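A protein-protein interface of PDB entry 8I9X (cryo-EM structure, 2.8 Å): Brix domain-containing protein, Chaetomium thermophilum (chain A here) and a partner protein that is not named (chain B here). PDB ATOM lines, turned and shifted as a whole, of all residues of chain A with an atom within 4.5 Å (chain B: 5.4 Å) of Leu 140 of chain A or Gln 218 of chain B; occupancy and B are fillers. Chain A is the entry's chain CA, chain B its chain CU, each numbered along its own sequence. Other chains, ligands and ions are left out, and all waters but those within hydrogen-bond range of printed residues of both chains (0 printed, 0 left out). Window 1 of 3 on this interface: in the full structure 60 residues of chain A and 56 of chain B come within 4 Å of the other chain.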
ATOM      1  N   ARG A 137      15.488 -13.967  18.365  1.00  0.00           N
ATOM      2  CA  ARG A 137      15.713 -12.765  17.550  1.00  0.00           C
ATOM      3  C   ARG A 137      17.007 -12.121  17.986  1.00  0.00           C
ATOM      4  O   ARG A 137      17.168 -11.854  19.175  1.00  0.00           O
ATOM      5  CB  ARG A 137      14.536 -11.823  17.746  1.00  0.00           C
ATOM      6  CG  ARG A 137      13.166 -12.398  17.438  1.00  0.00           C
ATOM      7  CD  ARG A 137      12.201 -11.235  17.361  1.00  0.00           C
ATOM      8  NE  ARG A 137      12.675 -10.270  16.383  1.00  0.00           N
ATOM      9  CZ  ARG A 137      12.501  -8.959  16.463  1.00  0.00           C
ATOM     10  NH1 ARG A 137      11.865  -8.438  17.494  1.00  0.00           N
ATOM     11  NH2 ARG A 137      12.968  -8.171  15.513  1.00  0.00           N
ATOM     12  N   PRO A 138      17.943 -11.882  17.068  1.00  0.00           N
ATOM     13  CA  PRO A 138      19.217 -11.369  17.473  1.00  0.00           C
ATOM     14  C   PRO A 138      19.334  -9.853  17.511  1.00  0.00           C
ATOM     15  O   PRO A 138      18.647  -9.202  16.758  1.00  0.00           O
ATOM     16  CB  PRO A 138      20.075 -11.884  16.322  1.00  0.00           C
ATOM     17  CG  PRO A 138      19.191 -11.844  15.107  1.00  0.00           C
ATOM     18  CD  PRO A 138      17.804 -12.114  15.638  1.00  0.00           C
ATOM     19  N   ILE A 139      20.136  -9.319  18.420  1.00  0.00           N
ATOM     20  CA  ILE A 139      20.418  -7.863  18.383  1.00  0.00           C
ATOM     21  C   ILE A 139      21.490  -7.730  17.315  1.00  0.00           C
ATOM     22  O   ILE A 139      22.507  -8.408  17.426  1.00  0.00           O
ATOM     23  CB  ILE A 139      20.870  -7.319  19.750  1.00  0.00           C
ATOM     24  CG1 ILE A 139      19.771  -7.474  20.802  1.00  0.00           C
ATOM     25  CG2 ILE A 139      21.342  -5.880  19.639  1.00  0.00           C
ATOM     26  CD1 ILE A 139      20.175  -7.021  22.178  1.00  0.00           C
ATOM     27  N   LEU A 140      21.244  -6.929  16.290  1.00  0.00           N
ATOM     28  CA  LEU A 140      22.214  -6.818  15.182  1.00  0.00           C
ATOM     29  C   LEU A 140      23.097  -5.614  15.475  1.00  0.00           C
ATOM     30  O   LEU A 140      22.561  -4.519  15.622  1.00  0.00           O
ATOM     31  CB  LEU A 140      21.482  -6.673  13.846  1.00  0.00           C
ATOM     32  CG  LEU A 140      20.798  -7.907  13.263  1.00  0.00           C
ATOM     33  CD1 LEU A 140      21.566  -9.175  13.586  1.00  0.00           C
ATOM     34  CD2 LEU A 140      19.356  -8.012  13.729  1.00  0.00           C
ATOM     35  N   SER A 141      24.402  -5.825  15.566  1.00  0.00           N
ATOM     36  CA  SER A 141      25.360  -4.731  15.842  1.00  0.00           C
ATOM     37  C   SER A 141      26.106  -4.391  14.563  1.00  0.00           C
ATOM     38  O   SER A 141      26.627  -5.311  13.924  1.00  0.00           O
ATOM     39  CB  SER A 141      26.326  -5.143  16.883  1.00  0.00           C
ATOM     40  OG  SER A 141      27.376  -4.196  16.997  1.00  0.00           O
ATOM     41  N   PHE A 142      26.153  -3.119  14.205  1.00  0.00           N
ATOM     42  CA  PHE A 142      26.830  -2.696  12.957  1.00  0.00           C
ATOM     43  C   PHE A 142      27.848  -1.611  13.301  1.00  0.00           C
ATOM     44  O   PHE A 142      27.531  -0.739  14.116  1.00  0.00           O
ATOM     45  CB  PHE A 142      25.794  -2.217  11.936  1.00  0.00           C
ATOM     46  CG  PHE A 142      24.812  -3.217  11.387  1.00  0.00           C
ATOM     47  CD1 PHE A 142      25.146  -4.023  10.314  1.00  0.00           C
ATOM     48  CD2 PHE A 142      23.528  -3.300  11.897  1.00  0.00           C
ATOM     49  CE1 PHE A 142      24.232  -4.921   9.792  1.00  0.00           C
ATOM     50  CE2 PHE A 142      22.616  -4.202  11.376  1.00  0.00           C
ATOM     51  CZ  PHE A 142      22.968  -5.010  10.324  1.00  0.00           C
ATOM     52  N   LEU A 160      20.160  -6.488   7.285  1.00  0.00           N
ATOM     53  CA  LEU A 160      19.037  -6.346   8.241  1.00  0.00           C
ATOM     54  C   LEU A 160      17.870  -7.208   7.764  1.00  0.00           C
ATOM     55  O   LEU A 160      17.262  -7.869   8.607  1.00  0.00           O
ATOM     56  CB  LEU A 160      18.649  -4.868   8.355  1.00  0.00           C
ATOM     57  CG  LEU A 160      17.625  -4.528   9.435  1.00  0.00           C
ATOM     58  CD1 LEU A 160      18.122  -4.954  10.807  1.00  0.00           C
ATOM     59  CD2 LEU A 160      17.299  -3.047   9.423  1.00  0.00           C
ATOM     60  N   PHE A 163      19.394 -11.226   8.226  1.00  0.00           N
ATOM     61  CA  PHE A 163      19.720 -11.706   9.587  1.00  0.00           C
ATOM     62  C   PHE A 163      18.844 -10.981  10.613  1.00  0.00           C
ATOM     63  O   PHE A 163      19.301 -10.827  11.744  1.00  0.00           O
ATOM     64  CB  PHE A 163      21.221 -11.550   9.840  1.00  0.00           C
ATOM     65  CG  PHE A 163      22.152 -12.241   8.884  1.00  0.00           C
ATOM     66  CD1 PHE A 163      22.292 -13.616   8.903  1.00  0.00           C
ATOM     67  CD2 PHE A 163      22.923 -11.512   7.996  1.00  0.00           C
ATOM     68  CE1 PHE A 163      23.160 -14.252   8.031  1.00  0.00           C
ATOM     69  CE2 PHE A 163      23.796 -12.147   7.132  1.00  0.00           C
ATOM     70  CZ  PHE A 163      23.911 -13.515   7.148  1.00  0.00           C
ATOM     71  N   GLY A 164      17.607 -10.632  10.271  1.00  0.00           N
ATOM     72  CA  GLY A 164      16.725  -9.840  11.141  1.00  0.00           C
ATOM     73  C   GLY A 164      15.726 -10.615  11.963  1.00  0.00           C
ATOM     74  O   GLY A 164      15.547 -10.161  13.107  1.00  0.00           O
ATOM     75  N   ILE A 176      15.581 -13.340  23.986  1.00  0.00           N
ATOM     76  CA  ILE A 176      16.713 -12.993  23.136  1.00  0.00           C
ATOM     77  C   ILE A 176      17.997 -13.111  23.944  1.00  0.00           C
ATOM     78  O   ILE A 176      18.085 -12.609  25.071  1.00  0.00           O
ATOM     79  CB  ILE A 176      16.548 -11.587  22.534  1.00  0.00           C
ATOM     80  CG1 ILE A 176      16.502 -10.525  23.623  1.00  0.00           C
ATOM     81  CG2 ILE A 176      15.270 -11.514  21.714  1.00  0.00           C
ATOM     82  CD1 ILE A 176      16.582  -9.141  23.083  1.00  0.00           C
ATOM     83  N   LEU A 180      24.635 -10.505  16.933  1.00  0.00           N
ATOM     84  CA  LEU A 180      25.350 -10.736  15.686  1.00  0.00           C
ATOM     85  C   LEU A 180      25.986  -9.420  15.263  1.00  0.00           C
ATOM     86  O   LEU A 180      25.277  -8.443  15.001  1.00  0.00           O
ATOM     87  CB  LEU A 180      24.403 -11.261  14.609  1.00  0.00           C
ATOM     88  CG  LEU A 180      25.014 -12.027  13.437  1.00  0.00           C
ATOM     89  CD1 LEU A 180      25.618 -13.337  13.905  1.00  0.00           C
ATOM     90  CD2 LEU A 180      23.967 -12.271  12.367  1.00  0.00           C
ATOM     91  N   PRO B 213       9.811   1.202  16.723  1.00  0.00           N
ATOM     92  CA  PRO B 213      10.425   0.747  17.975  1.00  0.00           C
ATOM     93  C   PRO B 213      11.635  -0.154  17.754  1.00  0.00           C
ATOM     94  O   PRO B 213      11.789  -0.872  16.752  1.00  0.00           O
ATOM     95  CB  PRO B 213       9.289  -0.004  18.672  1.00  0.00           C
ATOM     96  CG  PRO B 213       8.415  -0.462  17.572  1.00  0.00           C
ATOM     97  CD  PRO B 213       8.501   0.572  16.488  1.00  0.00           C
ATOM     98  N   PHE B 214      12.518  -0.107  18.750  1.00  0.00           N
ATOM     99  CA  PHE B 214      13.645  -1.022  18.794  1.00  0.00           C
ATOM    100  C   PHE B 214      13.198  -2.471  18.889  1.00  0.00           C
ATOM    101  O   PHE B 214      13.910  -3.352  18.406  1.00  0.00           O
ATOM    102  CB  PHE B 214      14.562  -0.685  19.968  1.00  0.00           C
ATOM    103  CG  PHE B 214      15.864  -1.418  19.939  1.00  0.00           C
ATOM    104  CD1 PHE B 214      16.893  -0.986  19.125  1.00  0.00           C
ATOM    105  CD2 PHE B 214      16.060  -2.544  20.716  1.00  0.00           C
ATOM    106  CE1 PHE B 214      18.092  -1.660  19.090  1.00  0.00           C
ATOM    107  CE2 PHE B 214      17.257  -3.219  20.684  1.00  0.00           C
ATOM    108  CZ  PHE B 214      18.276  -2.777  19.872  1.00  0.00           C
ATOM    109  N   SER B 215      12.045  -2.740  19.486  1.00  0.00           N
ATOM    110  CA  SER B 215      11.540  -4.105  19.426  1.00  0.00           C
ATOM    111  C   SER B 215      11.253  -4.537  18.023  1.00  0.00           C
ATOM    112  O   SER B 215      11.373  -5.724  17.702  1.00  0.00           O
ATOM    113  CB  SER B 215      10.279  -4.244  20.280  1.00  0.00           C
ATOM    114  OG  SER B 215       9.770  -5.565  20.231  1.00  0.00           O
ATOM    115  N   PHE B 216      10.880  -3.588  17.169  1.00  0.00           N
ATOM    116  CA  PHE B 216      10.642  -3.862  15.761  1.00  0.00           C
ATOM    117  C   PHE B 216      11.911  -4.060  14.958  1.00  0.00           C
ATOM    118  O   PHE B 216      11.960  -4.970  14.130  1.00  0.00           O
ATOM    119  CB  PHE B 216       9.827  -2.730  15.124  1.00  0.00           C
ATOM    120  CG  PHE B 216       9.585  -2.907  13.653  1.00  0.00           C
ATOM    121  CD1 PHE B 216       8.511  -3.654  13.204  1.00  0.00           C
ATOM    122  CD2 PHE B 216      10.418  -2.316  12.720  1.00  0.00           C
ATOM    123  CE1 PHE B 216       8.281  -3.817  11.857  1.00  0.00           C
ATOM    124  CE2 PHE B 216      10.191  -2.477  11.371  1.00  0.00           C
ATOM    125  CZ  PHE B 216       9.120  -3.228  10.940  1.00  0.00           C
ATOM    126  N   HIS B 217      12.940  -3.246  15.172  1.00  0.00           N
ATOM    127  CA  HIS B 217      14.104  -3.377  14.293  1.00  0.00           C
ATOM    128  C   HIS B 217      15.313  -4.052  14.932  1.00  0.00           C
ATOM    129  O   HIS B 217      15.950  -4.881  14.279  1.00  0.00           O
ATOM    130  CB  HIS B 217      14.480  -1.999  13.718  1.00  0.00           C
ATOM    131  CG  HIS B 217      15.144  -1.079  14.691  1.00  0.00           C
ATOM    132  ND1 HIS B 217      16.494  -1.119  14.956  1.00  0.00           N
ATOM    133  CD2 HIS B 217      14.639  -0.083  15.456  1.00  0.00           C
ATOM    134  CE1 HIS B 217      16.793  -0.191  15.847  1.00  0.00           C
ATOM    135  NE2 HIS B 217      15.684   0.452  16.168  1.00  0.00           N
ATOM    136  N   GLN B 218      15.644  -3.738  16.187  1.00  0.00           N
ATOM    137  CA  GLN B 218      16.725  -4.400  16.931  1.00  0.00           C
ATOM    138  C   GLN B 218      18.068  -4.328  16.207  1.00  0.00           C
ATOM    139  O   GLN B 218      18.816  -5.306  16.155  1.00  0.00           O
ATOM    140  CB  GLN B 218      16.379  -5.856  17.259  1.00  0.00           C
ATOM    141  CG  GLN B 218      15.488  -6.034  18.477  1.00  0.00           C
ATOM    142  CD  GLN B 218      15.451  -7.464  18.972  1.00  0.00           C
ATOM    143  OE1 GLN B 218      16.030  -8.360  18.364  1.00  0.00           O
ATOM    144  NE2 GLN B 218      14.768  -7.685  20.087  1.00  0.00           N
ATOM    145  N   SER B 219      18.387  -3.164  15.655  1.00  0.00           N
ATOM    146  CA  SER B 219      19.686  -2.913  15.054  1.00  0.00           C
ATOM    147  C   SER B 219      20.327  -1.698  15.709  1.00  0.00           C
ATOM    148  O   SER B 219      19.688  -0.654  15.861  1.00  0.00           O
ATOM    149  CB  SER B 219      19.565  -2.694  13.543  1.00  0.00           C
ATOM    150  OG  SER B 219      18.763  -1.562  13.255  1.00  0.00           O
ATOM    151  N   VAL B 220      21.593  -1.837  16.094  1.00  0.00           N
ATOM    152  CA  VAL B 220      22.334  -0.768  16.753  1.00  0.00           C
ATOM    153  C   VAL B 220      23.550  -0.438  15.902  1.00  0.00           C
ATOM    154  O   VAL B 220      24.290  -1.342  15.496  1.00  0.00           O
ATOM    155  CB  VAL B 220      22.766  -1.155  18.177  1.00  0.00           C
ATOM    156  CG1 VAL B 220      23.337   0.053  18.898  1.00  0.00           C
ATOM    157  CG2 VAL B 220      21.600  -1.736  18.949  1.00  0.00           C
ATOM    158  N   ALA B 250      26.644  -2.587  21.719  1.00  0.00           N
ATOM    159  CA  ALA B 250      25.353  -2.812  21.081  1.00  0.00           C
ATOM    160  C   ALA B 250      24.411  -3.589  21.992  1.00  0.00           C
ATOM    161  O   ALA B 250      23.225  -3.260  22.085  1.00  0.00           O
ATOM    162  CB  ALA B 250      25.540  -3.546  19.756  1.00  0.00           C
ATOM    163  N   LEU B 258      15.153  -2.401  25.126  1.00  0.00           N
ATOM    164  CA  LEU B 258      14.127  -3.434  25.149  1.00  0.00           C
ATOM    165  C   LEU B 258      13.475  -3.554  26.520  1.00  0.00           C
ATOM    166  O   LEU B 258      12.269  -3.802  26.611  1.00  0.00           O
ATOM    167  CB  LEU B 258      14.726  -4.767  24.710  1.00  0.00           C
ATOM    168  CG  LEU B 258      14.833  -4.904  23.190  1.00  0.00           C
ATOM    169  CD1 LEU B 258      16.031  -5.739  22.813  1.00  0.00           C
ATOM    170  CD2 LEU B 258      13.564  -5.495  22.606  1.00  0.00           C
ATOM    171  N   VAL B 263       9.878  -5.723  26.480  1.00  0.00           N
ATOM    172  CA  VAL B 263      10.051  -7.023  25.840  1.00  0.00           C
ATOM    173  C   VAL B 263      10.827  -7.921  26.799  1.00  0.00           C
ATOM    174  O   VAL B 263      11.818  -7.463  27.388  1.00  0.00           O
ATOM    175  CB  VAL B 263      10.784  -6.892  24.500  1.00  0.00           C
ATOM    176  CG1 VAL B 263      11.051  -8.264  23.898  1.00  0.00           C
ATOM    177  CG2 VAL B 263       9.980  -6.035  23.540  1.00  0.00           C
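The guanidinium group (NH1) of Arg 137 of chain A is in hydrogen-bond range of the backbone carbonyl oxygen (O) of Ser 215 of chain B.
The side-chain amide oxygen of Gln 218 of chain B sits close to the backbone carbonyl oxygen of Pro 138 of chain A.
The backbone NH of Leu 140 of chain A is in hydrogen-bond range of the backbone carbonyl oxygen of Gln 218 of chain B (2.9 Å).
The backbone carbonyl oxygen of Leu 140 of chain A sits at hydrogen-bond distance from the backbone NH of Val 220 of chain B, 2.9 Å away.
O of Val 220 of chain B is in hydrogen-bond range of N of Phe 142 of chain A, at 2.9 Å.
A ring nitrogen (ND1) of His 217 of chain B lies within hydrogen-bond range of the side-chain hydroxyl (OG) of Ser 219 of chain B, at 2.9 Å.
O of Leu 258 of chain B is in hydrogen-bond range of N of Val 263 of chain B, at 3.1 Å.
The backbone carbonyl oxygen (O) of Ile 139 of chain A is in hydrogen-bond range of the backbone NH (N) of Leu 180 of chain A (3.0 Å).
O of Leu 180 of chain A is in hydrogen-bond range of N of Ser 141 of chain A (2.8 Å).
Phe 216 of chain B touches Arg 137 of chain A.
Arg 137 of chain A touches Gln 218 of chain B.
Gln 218 of chain B touches Ile 139 of chain A.
Leu 140 of chain A touches Ser 219 of chain B (O to CA, 3.3 Å).
Val 220 of chain B touches Ser 141 of chain A.
Ala 250 of chain B touches Ser 141 of chain A.
Ser 219 of chain B touches Leu 160 of chain A.
Ile 176 of chain A touches Gln 218 of chain B.
CD1 of Leu 258 of chain B touches CD1 of Ile 176 of chain A, at 3.5 Å.
Of the printed residues of chain B, Arg 137 of chain A touches Ser 215 (2.8 Å), Phe 216 (3.6 Å) and Gln 218 (3.8 Å).
Leu 140 of chain A touches three residues of chain B.
Of the printed residues of chain B, Phe 142 of chain A touches Val 220.
Of the printed residues of chain B, Leu 160 of chain A touches Ser 219 (3.8 Å).
Printed residues of chain B within 4 Å of Ile 176 of chain A: Gln 218 (3.8 Å) and Leu 258 (3.5 Å).
Of the printed residues of chain A, Ala 250 of chain B touches Ser 141 (3.4 Å).
Hydrophobic or aromatic side chains of chain A that line the printed part of chain B: Leu 140, Phe 142, Leu 160 and Ile 176.
Among the printed residues, no Asp or Glu carboxylate lies within 4 Å of a Lys or Arg side-chain nitrogen of the other chain.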
